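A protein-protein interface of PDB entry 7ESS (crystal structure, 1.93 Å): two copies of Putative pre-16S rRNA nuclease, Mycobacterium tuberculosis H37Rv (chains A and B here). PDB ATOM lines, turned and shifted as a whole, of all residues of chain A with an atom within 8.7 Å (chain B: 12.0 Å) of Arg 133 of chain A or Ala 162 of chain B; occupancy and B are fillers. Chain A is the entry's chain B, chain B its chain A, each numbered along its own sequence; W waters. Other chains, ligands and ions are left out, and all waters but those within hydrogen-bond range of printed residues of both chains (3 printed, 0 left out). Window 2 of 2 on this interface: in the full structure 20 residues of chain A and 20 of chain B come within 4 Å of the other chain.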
ATOM      1  N   LEU A 127      14.748   5.410  17.783  1.00  0.00           N
ATOM      2  CA  LEU A 127      14.236   6.218  18.878  1.00  0.00           C
ATOM      3  C   LEU A 127      14.587   7.701  18.676  1.00  0.00           C
ATOM      4  O   LEU A 127      13.795   8.608  18.992  1.00  0.00           O
ATOM      5  CB  LEU A 127      14.800   5.701  20.203  1.00  0.00           C
ATOM      6  CG  LEU A 127      14.303   6.472  21.424  1.00  0.00           C
ATOM      7  CD1 LEU A 127      12.806   6.354  21.532  1.00  0.00           C
ATOM      8  CD2 LEU A 127      14.996   6.025  22.695  1.00  0.00           C
ATOM      9  N   ARG A 128      15.785   7.965  18.187  1.00  0.00           N
ATOM     10  CA  ARG A 128      16.186   9.323  17.974  1.00  0.00           C
ATOM     11  C   ARG A 128      15.378   9.950  16.837  1.00  0.00           C
ATOM     12  O   ARG A 128      14.966  11.092  16.969  1.00  0.00           O
ATOM     13  CB  ARG A 128      17.678   9.367  17.677  1.00  0.00           C
ATOM     14  CG  ARG A 128      18.508   9.027  18.897  1.00  0.00           C
ATOM     15  CD  ARG A 128      19.941   8.888  18.450  1.00  0.00           C
ATOM     16  NE  ARG A 128      20.663   8.400  19.577  1.00  0.00           N
ATOM     17  CZ  ARG A 128      21.454   7.337  19.560  1.00  0.00           C
ATOM     18  NH1 ARG A 128      21.876   6.830  18.405  1.00  0.00           N
ATOM     19  NH2 ARG A 128      21.827   6.832  20.714  1.00  0.00           N
ATOM     20  N   GLN A 129      15.139   9.181  15.778  1.00  0.00           N
ATOM     21  CA  GLN A 129      14.414   9.656  14.615  1.00  0.00           C
ATOM     22  C   GLN A 129      13.006  10.043  15.036  1.00  0.00           C
ATOM     23  O   GLN A 129      12.509  11.095  14.667  1.00  0.00           O
ATOM     24  CB  GLN A 129      14.341   8.592  13.512  1.00  0.00           C
ATOM     25  CG  GLN A 129      13.011   8.569  12.756  1.00  0.00           C
ATOM     26  CD  GLN A 129      13.085   9.183  11.379  1.00  0.00           C
ATOM     27  OE1 GLN A 129      13.602  10.281  11.190  1.00  0.00           O
ATOM     28  NE2 GLN A 129      12.570   8.457  10.398  1.00  0.00           N
ATOM     29  N   ALA A 130      12.388   9.154  15.792  1.00  0.00           N
ATOM     30  CA  ALA A 130      11.041   9.358  16.272  1.00  0.00           C
ATOM     31  C   ALA A 130      10.959  10.668  17.063  1.00  0.00           C
ATOM     32  O   ALA A 130       9.960  11.383  16.944  1.00  0.00           O
ATOM     33  CB  ALA A 130      10.626   8.171  17.111  1.00  0.00           C
ATOM     34  N   GLY A 131      12.014  10.992  17.829  1.00  0.00           N
ATOM     35  CA  GLY A 131      12.037  12.148  18.742  1.00  0.00           C
ATOM     36  C   GLY A 131      12.512  13.453  18.096  1.00  0.00           C
ATOM     37  O   GLY A 131      12.373  14.519  18.710  1.00  0.00           O
ATOM     38  N   VAL A 132      13.120  13.399  16.912  1.00  0.00           N
ATOM     39  CA  VAL A 132      13.680  14.616  16.239  1.00  0.00           C
ATOM     40  C   VAL A 132      12.525  15.593  15.977  1.00  0.00           C
ATOM     41  O   VAL A 132      11.569  15.238  15.351  1.00  0.00           O
ATOM     42  N   ARG A 133      12.618  16.812  16.465  1.00  0.00           N
ATOM     43  CA  ARG A 133      11.596  17.839  16.193  1.00  0.00           C
ATOM     44  C   ARG A 133      12.282  19.176  15.840  1.00  0.00           C
ATOM     45  O   ARG A 133      11.661  20.263  15.937  1.00  0.00           O
ATOM     46  CB  ARG A 133      10.655  18.030  17.391  1.00  0.00           C
ATOM     47  CG  ARG A 133       9.719  16.868  17.675  1.00  0.00           C
ATOM     48  CD  ARG A 133       8.613  16.747  16.636  1.00  0.00           C
ATOM     49  NE  ARG A 133       7.709  15.638  16.927  1.00  0.00           N
ATOM     50  CZ  ARG A 133       8.013  14.348  16.776  1.00  0.00           C
ATOM     51  NH1 ARG A 133       9.205  13.983  16.325  1.00  0.00           N
ATOM     52  NH2 ARG A 133       7.117  13.425  17.087  1.00  0.00           N
ATOM     53  N   ALA A 134      13.530  19.121  15.386  1.00  0.00           N
ATOM     54  CA  ALA A 134      14.294  20.348  15.181  1.00  0.00           C
ATOM     55  C   ALA A 134      15.542  20.025  14.366  1.00  0.00           C
ATOM     56  O   ALA A 134      16.153  18.959  14.538  1.00  0.00           O
ATOM     57  CB  ALA A 134      14.672  20.980  16.514  1.00  0.00           C
ATOM     58  N   SER A 135      15.954  20.998  13.574  1.00  0.00           N
ATOM     59  CA  SER A 135      17.110  20.849  12.688  1.00  0.00           C
ATOM     60  C   SER A 135      18.404  20.687  13.506  1.00  0.00           C
ATOM     61  O   SER A 135      19.286  19.899  13.102  1.00  0.00           O
ATOM     62  CB  SER A 135      17.184  22.001  11.697  1.00  0.00           C
ATOM     63  OG  SER A 135      16.326  21.741  10.583  1.00  0.00           O
ATOM     64  N   GLU A 136      18.483  21.367  14.663  1.00  0.00           N
ATOM     65  CA  GLU A 136      19.634  21.302  15.586  1.00  0.00           C
ATOM     66  C   GLU A 136      19.901  19.837  15.988  1.00  0.00           C
ATOM     67  O   GLU A 136      21.044  19.412  16.088  1.00  0.00           O
ATOM     68  N   GLN A 137      18.838  19.080  16.221  1.00  0.00           N
ATOM     69  CA  GLN A 137      18.935  17.704  16.662  1.00  0.00           C
ATOM     70  C   GLN A 137      19.417  16.865  15.471  1.00  0.00           C
ATOM     71  O   GLN A 137      20.383  16.105  15.592  1.00  0.00           O
ATOM     72  CB  GLN A 137      17.592  17.213  17.224  1.00  0.00           C
ATOM     73  CG  GLN A 137      17.068  18.046  18.401  1.00  0.00           C
ATOM     74  CD  GLN A 137      15.577  17.938  18.655  1.00  0.00           C
ATOM     75  OE1 GLN A 137      14.833  17.299  17.916  1.00  0.00           O
ATOM     76  NE2 GLN A 137      15.117  18.615  19.697  1.00  0.00           N
ATOM     77  N   ARG A 138      18.768  17.063  14.323  1.00  0.00           N
ATOM     78  CA  ARG A 138      18.992  16.250  13.135  1.00  0.00           C
ATOM     79  C   ARG A 138      20.443  16.402  12.659  1.00  0.00           C
ATOM     80  O   ARG A 138      20.986  15.470  12.098  1.00  0.00           O
ATOM     81  CB  ARG A 138      17.969  16.625  12.054  1.00  0.00           C
ATOM     82  CG  ARG A 138      18.188  15.930  10.721  1.00  0.00           C
ATOM     83  CD  ARG A 138      16.943  15.931   9.858  1.00  0.00           C
ATOM     84  NE  ARG A 138      15.956  14.944  10.275  1.00  0.00           N
ATOM     85  CZ  ARG A 138      14.806  14.720   9.644  1.00  0.00           C
ATOM     86  NH1 ARG A 138      14.500  15.410   8.557  1.00  0.00           N
ATOM     87  NH2 ARG A 138      13.971  13.806  10.104  1.00  0.00           N
ATOM     88  N   ARG B  11      12.943  10.101  35.882  1.00  0.00           N
ATOM     89  CA  ARG B  11      12.366   9.899  34.562  1.00  0.00           C
ATOM     90  C   ARG B  11      12.914  10.943  33.582  1.00  0.00           C
ATOM     91  O   ARG B  11      12.709  12.156  33.774  1.00  0.00           O
ATOM     92  CB  ARG B  11      10.841  10.005  34.614  1.00  0.00           C
ATOM     93  CG  ARG B  11      10.192   9.952  33.241  1.00  0.00           C
ATOM     94  CD  ARG B  11       8.718   9.544  33.283  1.00  0.00           C
ATOM     95  NE  ARG B  11       7.828  10.676  33.509  1.00  0.00           N
ATOM     96  CZ  ARG B  11       7.356  11.469  32.553  1.00  0.00           C
ATOM     97  NH1 ARG B  11       7.685  11.251  31.286  1.00  0.00           N
ATOM     98  NH2 ARG B  11       6.558  12.473  32.874  1.00  0.00           N
ATOM     99  N   PRO B  12      13.558  10.499  32.514  1.00  0.00           N
ATOM    100  CA  PRO B  12      14.107  11.505  31.573  1.00  0.00           C
ATOM    101  C   PRO B  12      13.006  12.384  30.960  1.00  0.00           C
ATOM    102  O   PRO B  12      11.947  11.869  30.501  1.00  0.00           O
ATOM    103  CB  PRO B  12      14.782  10.693  30.460  1.00  0.00           C
ATOM    104  CG  PRO B  12      15.051   9.341  31.082  1.00  0.00           C
ATOM    105  CD  PRO B  12      14.014   9.152  32.164  1.00  0.00           C
ATOM    106  N   GLY B  13      13.259  13.696  30.945  1.00  0.00           N
ATOM    107  CA  GLY B  13      12.326  14.654  30.351  1.00  0.00           C
ATOM    108  C   GLY B  13      11.088  14.910  31.201  1.00  0.00           C
ATOM    109  O   GLY B  13      10.106  15.498  30.709  1.00  0.00           O
ATOM    110  N   ASP B  14      11.092  14.472  32.459  1.00  0.00           N
ATOM    111  CA  ASP B  14       9.967  14.752  33.328  1.00  0.00           C
ATOM    112  C   ASP B  14       9.743  16.271  33.358  1.00  0.00           C
ATOM    113  O   ASP B  14      10.662  17.019  33.744  1.00  0.00           O
ATOM    114  CB  ASP B  14      10.261  14.200  34.713  1.00  0.00           C
ATOM    115  CG  ASP B  14       9.120  14.386  35.683  1.00  0.00           C
ATOM    116  OD1 ASP B  14       8.320  15.328  35.484  1.00  0.00           O
ATOM    117  OD2 ASP B  14       9.079  13.617  36.622  1.00  0.00           O
ATOM    118  N   PRO B  15       8.541  16.735  32.969  1.00  0.00           N
ATOM    119  CA  PRO B  15       8.379  18.191  32.859  1.00  0.00           C
ATOM    120  C   PRO B  15       8.534  18.880  34.218  1.00  0.00           C
ATOM    121  O   PRO B  15       8.916  20.033  34.262  1.00  0.00           O
ATOM    122  CB  PRO B  15       6.977  18.399  32.271  1.00  0.00           C
ATOM    123  CG  PRO B  15       6.732  17.123  31.516  1.00  0.00           C
ATOM    124  CD  PRO B  15       7.350  16.065  32.412  1.00  0.00           C
ATOM    125  N   ASP B  18      12.593  19.101  34.379  1.00  0.00           N
ATOM    126  CA  ASP B  18      13.465  19.373  33.262  1.00  0.00           C
ATOM    127  C   ASP B  18      13.806  20.874  33.208  1.00  0.00           C
ATOM    128  O   ASP B  18      12.927  21.689  33.130  1.00  0.00           O
ATOM    129  CB  ASP B  18      12.823  18.962  31.935  1.00  0.00           C
ATOM    130  CG  ASP B  18      13.852  18.898  30.822  1.00  0.00           C
ATOM    131  OD1 ASP B  18      14.405  17.803  30.610  1.00  0.00           O
ATOM    132  OD2 ASP B  18      14.156  19.954  30.247  1.00  0.00           O
ATOM    133  N   ASP B  42      22.448  21.823  23.015  1.00  0.00           N
ATOM    134  CA  ASP B  42      21.114  21.463  22.635  1.00  0.00           C
ATOM    135  C   ASP B  42      20.706  20.093  23.198  1.00  0.00           C
ATOM    136  O   ASP B  42      19.635  19.609  22.835  1.00  0.00           O
ATOM    137  CB  ASP B  42      21.002  21.514  21.110  1.00  0.00           C
ATOM    138  CG  ASP B  42      21.175  22.941  20.587  1.00  0.00           C
ATOM    139  OD1 ASP B  42      20.617  23.824  21.193  1.00  0.00           O
ATOM    140  OD2 ASP B  42      21.913  23.133  19.616  1.00  0.00           O
ATOM    141  N   ALA B  43      21.567  19.465  24.036  1.00  0.00           N
ATOM    142  CA  ALA B  43      21.260  18.216  24.780  1.00  0.00           C
ATOM    143  C   ALA B  43      20.817  17.072  23.850  1.00  0.00           C
ATOM    144  O   ALA B  43      19.834  16.379  24.141  1.00  0.00           O
ATOM    145  CB  ALA B  43      20.211  18.476  25.819  1.00  0.00           C
ATOM    146  N   ILE B  44      21.624  16.816  22.847  1.00  0.00           N
ATOM    147  CA  ILE B  44      21.359  15.776  21.841  1.00  0.00           C
ATOM    148  C   ILE B  44      22.431  14.683  21.874  1.00  0.00           C
ATOM    149  O   ILE B  44      22.112  13.534  21.586  1.00  0.00           O
ATOM    150  CB  ILE B  44      21.310  16.431  20.442  1.00  0.00           C
ATOM    151  CG1 ILE B  44      20.268  17.544  20.377  1.00  0.00           C
ATOM    152  CG2 ILE B  44      21.070  15.391  19.373  1.00  0.00           C
ATOM    153  CD1 ILE B  44      20.667  18.638  19.469  1.00  0.00           C
ATOM    154  N   TRP B 153      19.913   8.831  28.570  1.00  0.00           N
ATOM    155  CA  TRP B 153      19.109   9.880  29.177  1.00  0.00           C
ATOM    156  C   TRP B 153      18.676  10.895  28.101  1.00  0.00           C
ATOM    157  O   TRP B 153      17.478  11.261  28.022  1.00  0.00           O
ATOM    158  CB  TRP B 153      19.886  10.536  30.320  1.00  0.00           C
ATOM    159  CG  TRP B 153      19.128  11.652  30.983  1.00  0.00           C
ATOM    160  CD1 TRP B 153      19.031  12.950  30.571  1.00  0.00           C
ATOM    161  CD2 TRP B 153      18.249  11.517  32.100  1.00  0.00           C
ATOM    162  NE1 TRP B 153      18.242  13.653  31.435  1.00  0.00           N
ATOM    163  CE2 TRP B 153      17.753  12.803  32.394  1.00  0.00           C
ATOM    164  CE3 TRP B 153      17.917  10.454  32.945  1.00  0.00           C
ATOM    165  CZ2 TRP B 153      16.862  13.040  33.445  1.00  0.00           C
ATOM    166  CZ3 TRP B 153      17.057  10.694  33.997  1.00  0.00           C
ATOM    167  CH2 TRP B 153      16.545  11.979  34.246  1.00  0.00           C
ATOM    168  N   LEU B 154      19.597  11.320  27.225  1.00  0.00           N
ATOM    169  CA  LEU B 154      19.263  12.397  26.289  1.00  0.00           C
ATOM    170  C   LEU B 154      18.234  11.888  25.275  1.00  0.00           C
ATOM    171  O   LEU B 154      17.313  12.605  24.887  1.00  0.00           O
ATOM    172  CB  LEU B 154      20.503  12.854  25.513  1.00  0.00           C
ATOM    173  CG  LEU B 154      21.646  13.470  26.310  1.00  0.00           C
ATOM    174  CD1 LEU B 154      22.795  13.812  25.369  1.00  0.00           C
ATOM    175  CD2 LEU B 154      21.181  14.697  27.072  1.00  0.00           C
ATOM    176  N   ASP B 155      18.430  10.654  24.846  1.00  0.00           N
ATOM    177  CA  ASP B 155      17.536  10.005  23.880  1.00  0.00           C
ATOM    178  C   ASP B 155      16.120   9.856  24.459  1.00  0.00           C
ATOM    179  O   ASP B 155      15.112  10.137  23.777  1.00  0.00           O
ATOM    180  CB  ASP B 155      18.049   8.608  23.542  1.00  0.00           C
ATOM    181  CG  ASP B 155      19.330   8.581  22.725  1.00  0.00           C
ATOM    182  OD1 ASP B 155      19.729   9.644  22.184  1.00  0.00           O
ATOM    183  OD2 ASP B 155      19.967   7.503  22.693  1.00  0.00           O
ATOM    184  N   GLU B 156      16.047   9.324  25.674  1.00  0.00           N
ATOM    185  CA  GLU B 156      14.769   9.119  26.359  1.00  0.00           C
ATOM    186  C   GLU B 156      14.092  10.474  26.596  1.00  0.00           C
ATOM    187  O   GLU B 156      12.906  10.603  26.490  1.00  0.00           O
ATOM    188  CB  GLU B 156      14.985   8.393  27.694  1.00  0.00           C
ATOM    189  CG  GLU B 156      15.416   6.937  27.562  1.00  0.00           C
ATOM    190  CD  GLU B 156      14.415   6.006  26.868  1.00  0.00           C
ATOM    191  OE1 GLU B 156      13.207   6.339  26.771  1.00  0.00           O
ATOM    192  OE2 GLU B 156      14.845   4.951  26.417  1.00  0.00           O
ATOM    193  N   ARG B 157      14.859  11.486  26.955  1.00  0.00           N
ATOM    194  CA  ARG B 157      14.301  12.813  27.219  1.00  0.00           C
ATOM    195  C   ARG B 157      13.613  13.376  25.953  1.00  0.00           C
ATOM    196  O   ARG B 157      12.494  13.840  25.990  1.00  0.00           O
ATOM    197  CB  ARG B 157      15.438  13.735  27.687  1.00  0.00           C
ATOM    198  CG  ARG B 157      15.082  15.211  27.717  1.00  0.00           C
ATOM    199  CD  ARG B 157      16.205  16.081  28.257  1.00  0.00           C
ATOM    200  NE  ARG B 157      15.783  17.474  28.351  1.00  0.00           N
ATOM    201  CZ  ARG B 157      15.868  18.371  27.364  1.00  0.00           C
ATOM    202  NH1 ARG B 157      16.415  18.034  26.200  1.00  0.00           N
ATOM    203  NH2 ARG B 157      15.429  19.610  27.568  1.00  0.00           N
ATOM    204  N   LEU B 158      14.313  13.405  24.836  1.00  0.00           N
ATOM    205  CA  LEU B 158      13.748  13.952  23.603  1.00  0.00           C
ATOM    206  C   LEU B 158      12.507  13.140  23.203  1.00  0.00           C
ATOM    207  O   LEU B 158      11.550  13.713  22.727  1.00  0.00           O
ATOM    208  CB  LEU B 158      14.786  13.909  22.472  1.00  0.00           C
ATOM    209  CG  LEU B 158      15.416  15.237  22.014  1.00  0.00           C
ATOM    210  CD1 LEU B 158      15.171  16.419  22.953  1.00  0.00           C
ATOM    211  CD2 LEU B 158      16.920  15.055  21.813  1.00  0.00           C
ATOM    212  N   ALA B 159      12.537  11.833  23.427  1.00  0.00           N
ATOM    213  CA  ALA B 159      11.425  10.954  23.067  1.00  0.00           C
ATOM    214  C   ALA B 159      10.196  11.316  23.900  1.00  0.00           C
ATOM    215  O   ALA B 159       9.108  11.485  23.360  1.00  0.00           O
ATOM    216  CB  ALA B 159      11.804   9.517  23.273  1.00  0.00           C
ATOM    217  N   ALA B 160      10.404  11.450  25.199  1.00  0.00           N
ATOM    218  CA  ALA B 160       9.353  11.878  26.145  1.00  0.00           C
ATOM    219  C   ALA B 160       8.805  13.257  25.774  1.00  0.00           C
ATOM    220  O   ALA B 160       7.609  13.453  25.840  1.00  0.00           O
ATOM    221  CB  ALA B 160       9.884  11.868  27.552  1.00  0.00           C
ATOM    222  N   MET B 161       9.647  14.177  25.327  1.00  0.00           N
ATOM    223  CA  MET B 161       9.193  15.529  25.026  1.00  0.00           C
ATOM    224  C   MET B 161       8.397  15.571  23.713  1.00  0.00           C
ATOM    225  O   MET B 161       7.532  16.432  23.561  1.00  0.00           O
ATOM    226  CB  MET B 161      10.373  16.506  24.956  1.00  0.00           C
ATOM    227  CG  MET B 161      10.984  16.777  26.304  1.00  0.00           C
ATOM    228  SD  MET B 161      12.610  17.587  26.245  1.00  0.00           S
ATOM    229  CE  MET B 161      12.315  18.894  25.051  1.00  0.00           C
ATOM    230  N   ALA B 162       8.678  14.698  22.761  1.00  0.00           N
ATOM    231  CA  ALA B 162       8.024  14.722  21.459  1.00  0.00           C
ATOM    232  C   ALA B 162       6.541  14.354  21.587  1.00  0.00           C
ATOM    233  O   ALA B 162       6.224  13.279  22.091  1.00  0.00           O
ATOM    234  CB  ALA B 162       8.735  13.774  20.524  1.00  0.00           C
HETATM  235  O   HOH W   1      17.270  20.153  21.684  1.00  0.00           O
HETATM  236  O   HOH W   2      11.571  15.716  20.975  1.00  0.00           O
HETATM  237  O   HOH W   3      14.880  10.876  21.010  1.00  0.00           O
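The side-chain carboxylate (OD2) of Asp 155 of chain B is in salt-bridge range of the guanidinium group (NH2) of Arg 128 of chain A.
The side-chain amide oxygen (OE1) of Gln 137 of chain A lies within hydrogen-bond range of the backbone NH (N) of Ala 134 of chain A, 3.4 Å away. OE1 of Gln 137 of chain A is in hydrogen-bond range of N of Arg 133 of chain A, 2.7 Å away. O of Ala 130 of chain A sits at hydrogen-bond distance from NH1 of Arg 133 of chain A, at 2.8 Å.
Among the printed residues, merely in contact across the chains: Leu 127 of chain A with Glu 156 of chain B (3.9 Å), Leu 127 of chain A with Ala 159 of chain B (3.7 Å), Arg 133 of chain A with Ala 162 of chain B (3.8 Å), Glu 136 of chain A with Ile 44 of chain B (3.5 Å), Gln 137 of chain A with Ile 44 of chain B (3.4 Å) and Gln 137 of chain A with Leu 158 of chain B (3.9 Å).
Of the printed residues of chain B, Leu 127 of chain A touches Glu 156 and Ala 159. Of the printed residues of chain B, Arg 128 of chain A touches Asp 155. No residue of chain B comes within 4 Å of Gly 131 of chain A. Of chain B, only Ala 162 (3.8 Å) comes within 4 Å of Arg 133 of chain A. No residue of chain B comes within 4 Å of Ala 134 of chain A. Of the printed residues of chain B, Glu 136 of chain A touches Ile 44 (3.5 Å). Gln 137 of chain A touches just these residues of chain B: Ile 44 and Leu 158. Pro 12 of chain B touches none of the printed residues of chain A. Gly 13 of chain B touches none of the printed residues of chain A. Of the printed residues of chain A, Ile 44 of chain B touches Glu 136 and Gln 137. Of chain A, only Arg 133 comes within 4 Å of Ala 162 of chain B. The nearest residue of chain B that does not touch Arg 133 of chain A is Leu 158 of chain B (6.2 Å). The nearest residue of chain A that does not touch Ala 162 of chain B is Gly 131 of chain A (4.1 Å).
Of the 12 printed residues of chain A, 5 touch a printed residue of chain B. Printed residues of chain A that touch a printed residue of chain B: Leu 127, Arg 128, Arg 133, Glu 136 and Gln 137. Hydrophobic or aromatic side chains of chain A that line the printed part of chain B: Leu 127. Among the printed residues, 7 pairs touch across the chains. Among the printed residues, Asp or Glu carboxylates within 4 Å of a Lys or Arg side-chain nitrogen of the other chain: Arg 128 of chain A with Asp 155 of chain B (2.8 Å).
No position is printed for both chains. Of the 7 pairs that touch across the chains among the printed residues, none has its exchanged pair printed and touching as well.
Water W2 lies within hydrogen-bond range of O of Leu 158 of chain B (2.7 Å) and O of Gly 131 of chain A (2.7 Å). Water W1 lies within hydrogen-bond range of O of Asp 42 of chain B (2.7 Å) and NE2 of Gln 137 of chain A (3.3 Å). Water W3 lies within hydrogen-bond range of O of Asp 155 of chain B (2.9 Å), O of Leu 127 of chain A (3.2 Å) and N of Ala 159 of chain B (3.5 Å).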
